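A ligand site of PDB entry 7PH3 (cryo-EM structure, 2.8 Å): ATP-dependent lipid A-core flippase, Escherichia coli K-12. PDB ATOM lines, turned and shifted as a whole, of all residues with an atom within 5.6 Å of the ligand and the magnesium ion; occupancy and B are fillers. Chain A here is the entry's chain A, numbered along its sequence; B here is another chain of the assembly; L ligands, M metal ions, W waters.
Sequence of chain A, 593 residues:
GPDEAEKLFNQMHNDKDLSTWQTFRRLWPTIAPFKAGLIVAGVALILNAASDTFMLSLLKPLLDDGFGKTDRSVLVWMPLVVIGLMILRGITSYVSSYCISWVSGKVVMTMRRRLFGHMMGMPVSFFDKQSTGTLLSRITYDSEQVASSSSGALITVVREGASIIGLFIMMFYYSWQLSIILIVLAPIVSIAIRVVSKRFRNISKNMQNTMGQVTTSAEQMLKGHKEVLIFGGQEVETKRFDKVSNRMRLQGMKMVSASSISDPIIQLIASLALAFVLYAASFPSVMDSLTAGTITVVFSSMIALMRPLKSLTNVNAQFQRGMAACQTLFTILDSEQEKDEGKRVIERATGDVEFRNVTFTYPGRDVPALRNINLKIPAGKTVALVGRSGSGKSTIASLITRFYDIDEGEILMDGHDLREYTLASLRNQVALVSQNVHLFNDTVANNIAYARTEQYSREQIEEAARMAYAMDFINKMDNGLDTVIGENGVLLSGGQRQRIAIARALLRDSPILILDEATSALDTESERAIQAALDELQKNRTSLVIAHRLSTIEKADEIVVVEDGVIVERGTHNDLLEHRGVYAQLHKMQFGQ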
ATOM      1  N   ASP A 128      12.799 -36.008   3.209  1.00  0.00           N
ATOM      2  CA  ASP A 128      14.230 -35.904   2.936  1.00  0.00           C
ATOM      3  C   ASP A 128      14.810 -37.247   2.507  1.00  0.00           C
ATOM      4  O   ASP A 128      15.607 -37.319   1.567  1.00  0.00           O
ATOM      5  CB  ASP A 128      14.957 -35.355   4.154  1.00  0.00           C
ATOM      6  CG  ASP A 128      14.661 -33.896   4.397  1.00  0.00           C
ATOM      7  OD1 ASP A 128      13.810 -33.330   3.671  1.00  0.00           O
ATOM      8  OD2 ASP A 128      15.264 -33.310   5.320  1.00  0.00           O
ATOM      9  N   LYS A 129      14.401 -38.340   3.163  1.00  0.00           N
ATOM     10  CA  LYS A 129      14.924 -39.657   2.830  1.00  0.00           C
ATOM     11  C   LYS A 129      14.104 -40.413   1.796  1.00  0.00           C
ATOM     12  O   LYS A 129      14.411 -41.574   1.519  1.00  0.00           O
ATOM     13  CB  LYS A 129      15.022 -40.522   4.097  1.00  0.00           C
ATOM     14  CG  LYS A 129      16.128 -40.124   5.054  1.00  0.00           C
ATOM     15  CD  LYS A 129      17.414 -39.735   4.345  1.00  0.00           C
ATOM     16  CE  LYS A 129      18.235 -38.786   5.208  1.00  0.00           C
ATOM     17  NZ  LYS A 129      17.376 -37.848   5.971  1.00  0.00           N
ATOM     18  N   TYR A 362      20.928 -33.402  12.773  1.00  0.00           N
ATOM     19  CA  TYR A 362      20.042 -33.891  11.734  1.00  0.00           C
ATOM     20  C   TYR A 362      19.984 -35.421  11.786  1.00  0.00           C
ATOM     21  O   TYR A 362      20.945 -36.066  12.192  1.00  0.00           O
ATOM     22  CB  TYR A 362      20.518 -33.435  10.363  1.00  0.00           C
ATOM     23  CG  TYR A 362      20.059 -32.058   9.964  1.00  0.00           C
ATOM     24  CD1 TYR A 362      18.773 -31.832   9.498  1.00  0.00           C
ATOM     25  CD2 TYR A 362      20.923 -30.981  10.035  1.00  0.00           C
ATOM     26  CE1 TYR A 362      18.365 -30.584   9.133  1.00  0.00           C
ATOM     27  CE2 TYR A 362      20.521 -29.723   9.663  1.00  0.00           C
ATOM     28  CZ  TYR A 362      19.248 -29.534   9.210  1.00  0.00           C
ATOM     29  OH  TYR A 362      18.852 -28.268   8.840  1.00  0.00           O
ATOM     30  N   ARG A 365      23.193 -38.142  10.912  1.00  0.00           N
ATOM     31  CA  ARG A 365      24.315 -37.317  10.519  1.00  0.00           C
ATOM     32  C   ARG A 365      25.374 -37.193  11.607  1.00  0.00           C
ATOM     33  O   ARG A 365      26.451 -36.638  11.326  1.00  0.00           O
ATOM     34  CB  ARG A 365      23.832 -35.921  10.113  1.00  0.00           C
ATOM     35  CG  ARG A 365      24.802 -35.095   9.261  1.00  0.00           C
ATOM     36  CD  ARG A 365      25.080 -35.679   7.890  1.00  0.00           C
ATOM     37  NE  ARG A 365      23.877 -35.919   7.097  1.00  0.00           N
ATOM     38  CZ  ARG A 365      23.706 -36.963   6.288  1.00  0.00           C
ATOM     39  NH1 ARG A 365      22.575 -37.109   5.612  1.00  0.00           N
ATOM     40  NH2 ARG A 365      24.659 -37.869   6.152  1.00  0.00           N
ATOM     41  N   ALA A 369      24.440 -29.814  14.153  1.00  0.00           N
ATOM     42  CA  ALA A 369      24.355 -28.627  13.329  1.00  0.00           C
ATOM     43  C   ALA A 369      24.307 -27.353  14.159  1.00  0.00           C
ATOM     44  O   ALA A 369      24.815 -26.323  13.720  1.00  0.00           O
ATOM     45  CB  ALA A 369      23.131 -28.699  12.419  1.00  0.00           C
ATOM     46  N   GLY A 387      26.342 -15.080   8.745  1.00  0.00           N
ATOM     47  CA  GLY A 387      27.351 -16.117   8.828  1.00  0.00           C
ATOM     48  C   GLY A 387      27.569 -16.740   7.477  1.00  0.00           C
ATOM     49  O   GLY A 387      26.777 -16.606   6.553  1.00  0.00           O
ATOM     50  N   ARG A 388      28.680 -17.461   7.360  1.00  0.00           N
ATOM     51  CA  ARG A 388      29.043 -18.099   6.115  1.00  0.00           C
ATOM     52  C   ARG A 388      28.054 -19.215   5.761  1.00  0.00           C
ATOM     53  O   ARG A 388      27.227 -19.629   6.559  1.00  0.00           O
ATOM     54  CB  ARG A 388      30.451 -18.649   6.185  1.00  0.00           C
ATOM     55  CG  ARG A 388      31.438 -17.746   6.840  1.00  0.00           C
ATOM     56  CD  ARG A 388      32.823 -18.246   6.582  1.00  0.00           C
ATOM     57  NE  ARG A 388      33.197 -17.999   5.188  1.00  0.00           N
ATOM     58  CZ  ARG A 388      34.246 -18.545   4.605  1.00  0.00           C
ATOM     59  NH1 ARG A 388      34.502 -18.275   3.334  1.00  0.00           N
ATOM     60  NH2 ARG A 388      35.034 -19.365   5.281  1.00  0.00           N
ATOM     61  N   SER A 389      28.175 -19.692   4.530  1.00  0.00           N
ATOM     62  CA  SER A 389      27.334 -20.767   4.059  1.00  0.00           C
ATOM     63  C   SER A 389      27.607 -22.042   4.832  1.00  0.00           C
ATOM     64  O   SER A 389      28.764 -22.370   5.124  1.00  0.00           O
ATOM     65  CB  SER A 389      27.546 -20.992   2.572  1.00  0.00           C
ATOM     66  OG  SER A 389      27.127 -19.872   1.828  1.00  0.00           O
ATOM     67  N   GLY A 390      26.541 -22.758   5.180  1.00  0.00           N
ATOM     68  CA  GLY A 390      26.640 -23.985   5.934  1.00  0.00           C
ATOM     69  C   GLY A 390      26.825 -23.829   7.416  1.00  0.00           C
ATOM     70  O   GLY A 390      27.180 -24.800   8.087  1.00  0.00           O
ATOM     71  N   SER A 391      26.588 -22.640   7.971  1.00  0.00           N
ATOM     72  CA  SER A 391      26.806 -22.404   9.390  1.00  0.00           C
ATOM     73  C   SER A 391      25.615 -22.800  10.256  1.00  0.00           C
ATOM     74  O   SER A 391      25.801 -23.075  11.446  1.00  0.00           O
ATOM     75  CB  SER A 391      27.160 -20.944   9.646  1.00  0.00           C
ATOM     76  OG  SER A 391      26.190 -20.073   9.106  1.00  0.00           O
ATOM     77  N   GLY A 392      24.403 -22.813   9.709  1.00  0.00           N
ATOM     78  CA  GLY A 392      23.272 -23.284  10.469  1.00  0.00           C
ATOM     79  C   GLY A 392      22.141 -22.312  10.673  1.00  0.00           C
ATOM     80  O   GLY A 392      21.403 -22.413  11.649  1.00  0.00           O
ATOM     81  N   LYS A 393      21.979 -21.357   9.751  1.00  0.00           N
ATOM     82  CA  LYS A 393      20.930 -20.358   9.873  1.00  0.00           C
ATOM     83  C   LYS A 393      19.571 -20.915   9.472  1.00  0.00           C
ATOM     84  O   LYS A 393      18.576 -20.767  10.205  1.00  0.00           O
ATOM     85  CB  LYS A 393      21.287 -19.135   9.038  1.00  0.00           C
ATOM     86  CG  LYS A 393      22.717 -18.662   9.249  1.00  0.00           C
ATOM     87  CD  LYS A 393      23.097 -17.518   8.326  1.00  0.00           C
ATOM     88  CE  LYS A 393      23.220 -17.979   6.883  1.00  0.00           C
ATOM     89  NZ  LYS A 393      24.568 -18.471   6.553  1.00  0.00           N
ATOM     90  N   SER A 394      19.493 -21.559   8.306  1.00  0.00           N
ATOM     91  CA  SER A 394      18.245 -22.203   7.902  1.00  0.00           C
ATOM     92  C   SER A 394      17.860 -23.305   8.865  1.00  0.00           C
ATOM     93  O   SER A 394      16.672 -23.623   9.000  1.00  0.00           O
ATOM     94  CB  SER A 394      18.370 -22.757   6.480  1.00  0.00           C
ATOM     95  OG  SER A 394      18.868 -21.786   5.585  1.00  0.00           O
ATOM     96  N   THR A 395      18.829 -23.904   9.549  1.00  0.00           N
ATOM     97  CA  THR A 395      18.516 -24.886  10.574  1.00  0.00           C
ATOM     98  C   THR A 395      17.766 -24.261  11.734  1.00  0.00           C
ATOM     99  O   THR A 395      16.779 -24.818  12.215  1.00  0.00           O
ATOM    100  CB  THR A 395      19.800 -25.558  11.051  1.00  0.00           C
ATOM    101  OG1 THR A 395      20.348 -26.343   9.988  1.00  0.00           O
ATOM    102  CG2 THR A 395      19.524 -26.468  12.227  1.00  0.00           C
ATOM    103  N   ILE A 396      18.213 -23.093  12.206  1.00  0.00           N
ATOM    104  CA  ILE A 396      17.479 -22.390  13.262  1.00  0.00           C
ATOM    105  C   ILE A 396      16.083 -22.036  12.778  1.00  0.00           C
ATOM    106  O   ILE A 396      15.080 -22.247  13.490  1.00  0.00           O
ATOM    107  CB  ILE A 396      18.275 -21.140  13.698  1.00  0.00           C
ATOM    108  CG1 ILE A 396      19.598 -21.554  14.318  1.00  0.00           C
ATOM    109  CG2 ILE A 396      17.475 -20.308  14.667  1.00  0.00           C
ATOM    110  CD1 ILE A 396      20.560 -20.423  14.541  1.00  0.00           C
ATOM    111  N   TYR A 404      11.891 -30.008  12.353  1.00  0.00           N
ATOM    112  CA  TYR A 404      12.642 -31.004  13.089  1.00  0.00           C
ATOM    113  C   TYR A 404      12.528 -30.681  14.563  1.00  0.00           C
ATOM    114  O   TYR A 404      12.210 -29.555  14.956  1.00  0.00           O
ATOM    115  CB  TYR A 404      14.110 -31.025  12.677  1.00  0.00           C
ATOM    116  CG  TYR A 404      14.331 -30.999  11.195  1.00  0.00           C
ATOM    117  CD1 TYR A 404      14.433 -29.804  10.516  1.00  0.00           C
ATOM    118  CD2 TYR A 404      14.443 -32.173  10.484  1.00  0.00           C
ATOM    119  CE1 TYR A 404      14.621 -29.774   9.157  1.00  0.00           C
ATOM    120  CE2 TYR A 404      14.638 -32.151   9.133  1.00  0.00           C
ATOM    121  CZ  TYR A 404      14.731 -30.955   8.474  1.00  0.00           C
ATOM    122  OH  TYR A 404      14.926 -30.933   7.124  1.00  0.00           O
ATOM    123  N   GLN A 435      14.564 -20.110   1.794  1.00  0.00           N
ATOM    124  CA  GLN A 435      15.698 -19.892   0.905  1.00  0.00           C
ATOM    125  C   GLN A 435      15.405 -20.391  -0.496  1.00  0.00           C
ATOM    126  O   GLN A 435      15.757 -19.742  -1.481  1.00  0.00           O
ATOM    127  CB  GLN A 435      16.953 -20.568   1.473  1.00  0.00           C
ATOM    128  CG  GLN A 435      18.211 -20.199   0.727  1.00  0.00           C
ATOM    129  CD  GLN A 435      19.454 -20.536   1.494  1.00  0.00           C
ATOM    130  OE1 GLN A 435      19.423 -21.295   2.450  1.00  0.00           O
ATOM    131  NE2 GLN A 435      20.569 -19.958   1.076  1.00  0.00           N
ATOM    132  N   ASP A 516      14.361 -15.853   4.707  1.00  0.00           N
ATOM    133  CA  ASP A 516      15.529 -16.705   4.563  1.00  0.00           C
ATOM    134  C   ASP A 516      16.210 -16.328   3.246  1.00  0.00           C
ATOM    135  O   ASP A 516      15.949 -16.943   2.211  1.00  0.00           O
ATOM    136  CB  ASP A 516      15.128 -18.172   4.601  1.00  0.00           C
ATOM    137  CG  ASP A 516      16.271 -19.096   4.943  1.00  0.00           C
ATOM    138  OD1 ASP A 516      17.294 -18.614   5.463  1.00  0.00           O
ATOM    139  OD2 ASP A 516      16.152 -20.307   4.683  1.00  0.00           O
ATOM    140  N   GLU A 517      17.067 -15.314   3.293  1.00  0.00           N
ATOM    141  CA  GLU A 517      17.725 -14.772   2.115  1.00  0.00           C
ATOM    142  C   GLU A 517      16.693 -14.379   1.053  1.00  0.00           C
ATOM    143  O   GLU A 517      16.724 -14.843  -0.087  1.00  0.00           O
ATOM    144  CB  GLU A 517      18.760 -15.747   1.557  1.00  0.00           C
ATOM    145  CG  GLU A 517      19.932 -15.940   2.476  1.00  0.00           C
ATOM    146  CD  GLU A 517      20.907 -16.958   1.956  1.00  0.00           C
ATOM    147  OE1 GLU A 517      20.776 -17.352   0.772  1.00  0.00           O
ATOM    148  OE2 GLU A 517      21.809 -17.360   2.722  1.00  0.00           O
ATOM    149  N   ILE A 546      17.535 -13.740   7.697  1.00  0.00           N
ATOM    150  CA  ILE A 546      18.759 -14.461   7.381  1.00  0.00           C
ATOM    151  C   ILE A 546      19.316 -13.840   6.112  1.00  0.00           C
ATOM    152  O   ILE A 546      18.706 -13.939   5.043  1.00  0.00           O
ATOM    153  CB  ILE A 546      18.507 -15.961   7.203  1.00  0.00           C
ATOM    154  CG1 ILE A 546      18.166 -16.609   8.538  1.00  0.00           C
ATOM    155  CG2 ILE A 546      19.710 -16.616   6.592  1.00  0.00           C
ATOM    156  CD1 ILE A 546      17.076 -17.624   8.437  1.00  0.00           C
ATOM    157  N   HIS A 548      22.900 -12.770   3.652  1.00  0.00           N
ATOM    158  CA  HIS A 548      24.343 -12.936   3.338  1.00  0.00           C
ATOM    159  C   HIS A 548      24.837 -11.548   2.938  1.00  0.00           C
ATOM    160  O   HIS A 548      26.058 -11.374   2.752  1.00  0.00           O
ATOM    161  CB  HIS A 548      24.540 -13.975   2.220  1.00  0.00           C
ATOM    162  CG  HIS A 548      24.960 -15.314   2.709  1.00  0.00           C
ATOM    163  ND1 HIS A 548      26.042 -15.488   3.556  1.00  0.00           N
ATOM    164  CD2 HIS A 548      24.468 -16.550   2.476  1.00  0.00           C
ATOM    165  CE1 HIS A 548      26.183 -16.763   3.818  1.00  0.00           C
ATOM    166  NE2 HIS A 548      25.229 -17.433   3.177  1.00  0.00           N
ATOM    167  N   VAL B 490      18.580 -31.668  -0.915  1.00  0.00           N
ATOM    168  CA  VAL B 490      17.910 -31.124   0.252  1.00  0.00           C
ATOM    169  C   VAL B 490      18.741 -31.285   1.510  1.00  0.00           C
ATOM    170  O   VAL B 490      18.588 -30.500   2.450  1.00  0.00           O
ATOM    171  CB  VAL B 490      16.506 -31.758   0.407  1.00  0.00           C
ATOM    172  CG1 VAL B 490      16.597 -33.243   0.702  1.00  0.00           C
ATOM    173  CG2 VAL B 490      15.699 -31.062   1.488  1.00  0.00           C
ATOM    174  N   LEU B 491      19.632 -32.257   1.551  1.00  0.00           N
ATOM    175  CA  LEU B 491      20.459 -32.467   2.726  1.00  0.00           C
ATOM    176  C   LEU B 491      21.687 -31.579   2.763  1.00  0.00           C
ATOM    177  O   LEU B 491      22.631 -31.874   3.484  1.00  0.00           O
ATOM    178  CB  LEU B 491      20.862 -33.939   2.824  1.00  0.00           C
ATOM    179  CG  LEU B 491      19.714 -34.954   2.731  1.00  0.00           C
ATOM    180  CD1 LEU B 491      20.178 -36.323   3.133  1.00  0.00           C
ATOM    181  CD2 LEU B 491      18.534 -34.539   3.586  1.00  0.00           C
ATOM    182  N   LEU B 492      21.669 -30.500   1.990  1.00  0.00           N
ATOM    183  CA  LEU B 492      22.744 -29.520   1.928  1.00  0.00           C
ATOM    184  C   LEU B 492      22.182 -28.138   2.161  1.00  0.00           C
ATOM    185  O   LEU B 492      20.981 -27.898   1.990  1.00  0.00           O
ATOM    186  CB  LEU B 492      23.449 -29.541   0.563  1.00  0.00           C
ATOM    187  CG  LEU B 492      24.284 -30.754   0.156  1.00  0.00           C
ATOM    188  CD1 LEU B 492      24.235 -30.903  -1.327  1.00  0.00           C
ATOM    189  CD2 LEU B 492      25.706 -30.550   0.613  1.00  0.00           C
ATOM    190  N   SER B 493      23.046 -27.220   2.556  1.00  0.00           N
ATOM    191  CA  SER B 493      22.655 -25.827   2.636  1.00  0.00           C
ATOM    192  C   SER B 493      22.572 -25.231   1.227  1.00  0.00           C
ATOM    193  O   SER B 493      23.016 -25.821   0.253  1.00  0.00           O
ATOM    194  CB  SER B 493      23.616 -25.054   3.527  1.00  0.00           C
ATOM    195  OG  SER B 493      24.652 -24.440   2.794  1.00  0.00           O
ATOM    196  N   GLY B 494      21.970 -24.047   1.135  1.00  0.00           N
ATOM    197  CA  GLY B 494      21.766 -23.431  -0.173  1.00  0.00           C
ATOM    198  C   GLY B 494      23.060 -23.087  -0.871  1.00  0.00           C
ATOM    199  O   GLY B 494      23.224 -23.355  -2.073  1.00  0.00           O
ATOM    200  N   GLY B 495      23.995 -22.477  -0.142  1.00  0.00           N
ATOM    201  CA  GLY B 495      25.286 -22.173  -0.726  1.00  0.00           C
ATOM    202  C   GLY B 495      26.064 -23.403  -1.108  1.00  0.00           C
ATOM    203  O   GLY B 495      26.799 -23.396  -2.096  1.00  0.00           O
ATOM    204  N   GLN B 496      25.917 -24.478  -0.343  1.00  0.00           N
ATOM    205  CA  GLN B 496      26.565 -25.729  -0.685  1.00  0.00           C
ATOM    206  C   GLN B 496      26.017 -26.305  -1.983  1.00  0.00           C
ATOM    207  O   GLN B 496      26.771 -26.807  -2.818  1.00  0.00           O
ATOM    208  CB  GLN B 496      26.421 -26.711   0.471  1.00  0.00           C
ATOM    209  CG  GLN B 496      27.132 -26.244   1.712  1.00  0.00           C
ATOM    210  CD  GLN B 496      27.039 -27.216   2.842  1.00  0.00           C
ATOM    211  OE1 GLN B 496      26.178 -28.080   2.849  1.00  0.00           O
ATOM    212  NE2 GLN B 496      27.930 -27.092   3.798  1.00  0.00           N
ATOM    213  N   ALA B 521      23.660 -17.364  -3.252  1.00  0.00           N
ATOM    214  CA  ALA B 521      23.454 -17.985  -1.945  1.00  0.00           C
ATOM    215  C   ALA B 521      24.734 -18.052  -1.125  1.00  0.00           C
ATOM    216  O   ALA B 521      24.749 -18.717  -0.084  1.00  0.00           O
ATOM    217  CB  ALA B 521      22.863 -19.379  -2.126  1.00  0.00           C
ATOM    218  N   LEU B 522      25.788 -17.381  -1.556  1.00  0.00           N
ATOM    219  CA  LEU B 522      27.099 -17.497  -0.961  1.00  0.00           C
ATOM    220  C   LEU B 522      27.451 -16.246  -0.178  1.00  0.00           C
ATOM    221  O   LEU B 522      26.873 -15.174  -0.376  1.00  0.00           O
ATOM    222  CB  LEU B 522      28.161 -17.747  -2.042  1.00  0.00           C
ATOM    223  CG  LEU B 522      28.044 -19.092  -2.742  1.00  0.00           C
ATOM    224  CD1 LEU B 522      29.096 -19.232  -3.798  1.00  0.00           C
ATOM    225  CD2 LEU B 522      28.142 -20.213  -1.728  1.00  0.00           C
HETATM  226  P1  LIG L   1      23.383 -20.790   3.597  1.00  0.00           P
HETATM  227  O1  LIG L   1      23.462 -19.411   4.169  1.00  0.00           O
HETATM  228  O2  LIG L   1      24.295 -20.850   2.408  1.00  0.00           O
HETATM  229  O3  LIG L   1      21.999 -21.059   3.106  1.00  0.00           O
HETATM  230  P2  LIG L   1      22.873 -22.111   6.105  1.00  0.00           P
HETATM  231  O4  LIG L   1      23.434 -21.349   7.271  1.00  0.00           O
HETATM  232  O5  LIG L   1      21.407 -21.960   5.777  1.00  0.00           O
HETATM  233  N1  LIG L   1      23.768 -21.860   4.760  1.00  0.00           N
HETATM  234  P3  LIG L   1      22.062 -24.753   6.975  1.00  0.00           P
HETATM  235  O6  LIG L   1      21.428 -24.298   8.247  1.00  0.00           O
HETATM  236  O7  LIG L   1      21.132 -25.001   5.835  1.00  0.00           O
HETATM  237  O8  LIG L   1      23.125 -23.656   6.497  1.00  0.00           O
HETATM  238  O9  LIG L   1      22.866 -26.057   7.234  1.00  0.00           O
HETATM  239  C1  LIG L   1      23.834 -26.201   8.308  1.00  0.00           C
HETATM  240  C2  LIG L   1      24.561 -27.507   8.163  1.00  0.00           C
HETATM  241  O10 LIG L   1      23.592 -28.591   8.156  1.00  0.00           O
HETATM  242  C3  LIG L   1      25.375 -27.686   6.880  1.00  0.00           C
HETATM  243  O11 LIG L   1      26.510 -28.514   7.110  1.00  0.00           O
HETATM  244  C4  LIG L   1      24.368 -28.398   5.970  1.00  0.00           C
HETATM  245  O12 LIG L   1      24.954 -29.124   4.912  1.00  0.00           O
HETATM  246  C5  LIG L   1      23.680 -29.326   6.957  1.00  0.00           C
HETATM  247  N2  LIG L   1      22.316 -29.669   6.553  1.00  0.00           N
HETATM  248  C6  LIG L   1      21.372 -28.800   6.045  1.00  0.00           C
HETATM  249  N3  LIG L   1      20.230 -29.394   5.791  1.00  0.00           N
HETATM  250  C7  LIG L   1      20.439 -30.722   6.128  1.00  0.00           C
HETATM  251  C8  LIG L   1      19.604 -31.851   6.086  1.00  0.00           C
HETATM  252  N4  LIG L   1      18.346 -31.827   5.658  1.00  0.00           N
HETATM  253  N5  LIG L   1      20.132 -33.033   6.503  1.00  0.00           N
HETATM  254  C9  LIG L   1      21.404 -33.054   6.932  1.00  0.00           C
HETATM  255  N6  LIG L   1      22.272 -32.049   7.029  1.00  0.00           N
HETATM  256  C10 LIG L   1      21.722 -30.902   6.614  1.00  0.00           C
HETATM  257 MG    MG M   1      20.296 -21.089   4.276  1.00  0.00          MG
HETATM  258  O   HOH W   1      20.194 -19.108   4.852  1.00  0.00           O
HETATM  259  O   HOH W   2      20.121 -23.131   4.082  1.00  0.00           O
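Within 4 Å of the magnesium ion: Ser 394 and Gln 435.
The nearest printed residue that does not touch the magnesium ion is Asp 516 (4.1 Å).
The backbone NH (N) of Gly 390 sits close to a nitrogen (N1) of the ligand, at 2.9 Å.
The backbone carbonyl oxygen (O) of Ala 521 of chain B sits close to an oxygen (O2) of the ligand (3.3 Å).
Residues that only touch the ligand: Tyr 362 (3.5 Å), Arg 365 (3.8 Å), Tyr 404 (3.8 Å), Leu 491 of chain B (3.4 Å), Leu 492 of chain B (3.7 Å) and Gly 494 of chain B (3.6 Å).
Hydrophobic or aromatic side chains within 4 Å of the ligand: Tyr 362, His 548 and Leu 491 of chain B.
Of the 30 residues printed, 22 come within 4 Å of the ligand.
The side-chain amide nitrogen (NE2) of Gln 435 lies within hydrogen-bond range of the side-chain carboxylate (OE1) of Glu 517, 2.6 Å away.
The backbone NH of Gln 435 is in hydrogen-bond range of the side-chain carboxylate of Asp 516, 3.3 Å away.
The side-chain carboxylate (OD2) of Asp 516 sits close to the side-chain hydroxyl (OG) of Ser 394 (3.2 Å).
The side-chain amino group of Lys 393 lies within hydrogen-bond range of the side-chain hydroxyl of Ser 391 (3.4 Å).
NE2 of His 548 sits close to OE2 of Glu 517 (3.5 Å).
A ring nitrogen (NE2) of His 548 sits at hydrogen-bond distance from the side-chain hydroxyl (OG) of Ser 389, at 3.4 Å.
ND1 of His 548 lies close to O of Gly 387 (3.3 Å).
The side-chain hydroxyl of Ser 389 is in hydrogen-bond range of the backbone carbonyl oxygen of Ala 521 of chain B (3.3 Å).
Water W1 lies within hydrogen-bond range of the side-chain carboxylate of Asp 516, the side-chain carboxylate of Glu 517 and an oxygen (O1) of the ligand.
The magnesium ion is bound by the side-chain amide oxygen (OE1) of Gln 435 (2.0 Å), water W2 (2.1 Å), the side-chain hydroxyl (OG) of Ser 394 (2.1 Å), an oxygen (O5) of the ligand (2.1 Å), an oxygen (O3) of the ligand (2.1 Å) and water W1 (2.1 Å).
The backbone NH (N) of Ser 394 sits at hydrogen-bond distance from an oxygen (O6) of the ligand (3.4 Å).
OE1 of Gln 496 of chain B is in hydrogen-bond range of O12 of the ligand, 2.6 Å away.
An oxygen (O4) of the ligand sits at hydrogen-bond distance from the backbone NH (N) of Lys 393, at 2.9 Å.
The side-chain amino group (NZ) of Lys 393 lies within salt-bridge range of an oxygen (O1) of the ligand, at 2.8 Å.
A ring nitrogen (NE2) of His 548 sits at hydrogen-bond distance from an oxygen (O1) of the ligand.
An oxygen (O6) of the ligand lies within hydrogen-bond range of the backbone NH (N) of Thr 395 (2.9 Å).
The side-chain hydroxyl (OG1) of Thr 395 sits at hydrogen-bond distance from an oxygen (O6) of the ligand, 2.9 Å away.
N of Gly 392 is in hydrogen-bond range of O4 of the ligand (3.0 Å).
An oxygen (O1) of the ligand sits close to the side-chain carboxylate (OE2) of Glu 517 (3.0 Å).
The backbone NH of Gly 495 of chain B lies within hydrogen-bond range of an oxygen (O2) of the ligand, 3.0 Å away.
OG of Ser 389 is in hydrogen-bond range of O2 of the ligand (3.1 Å).
The side-chain hydroxyl (OG) of Ser 493 of chain B sits at hydrogen-bond distance from a nitrogen (N1) of the ligand (3.4 Å).
A nitrogen (N4) of the ligand sits at hydrogen-bond distance from the side-chain carboxylate (OD2) of Asp 128, at 3.4 Å.
O4 of the ligand sits at hydrogen-bond distance from N of Ser 391 (3.5 Å).
N4 of the ligand is in hydrogen-bond range of O of Val 490 of chain B (3.5 Å).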
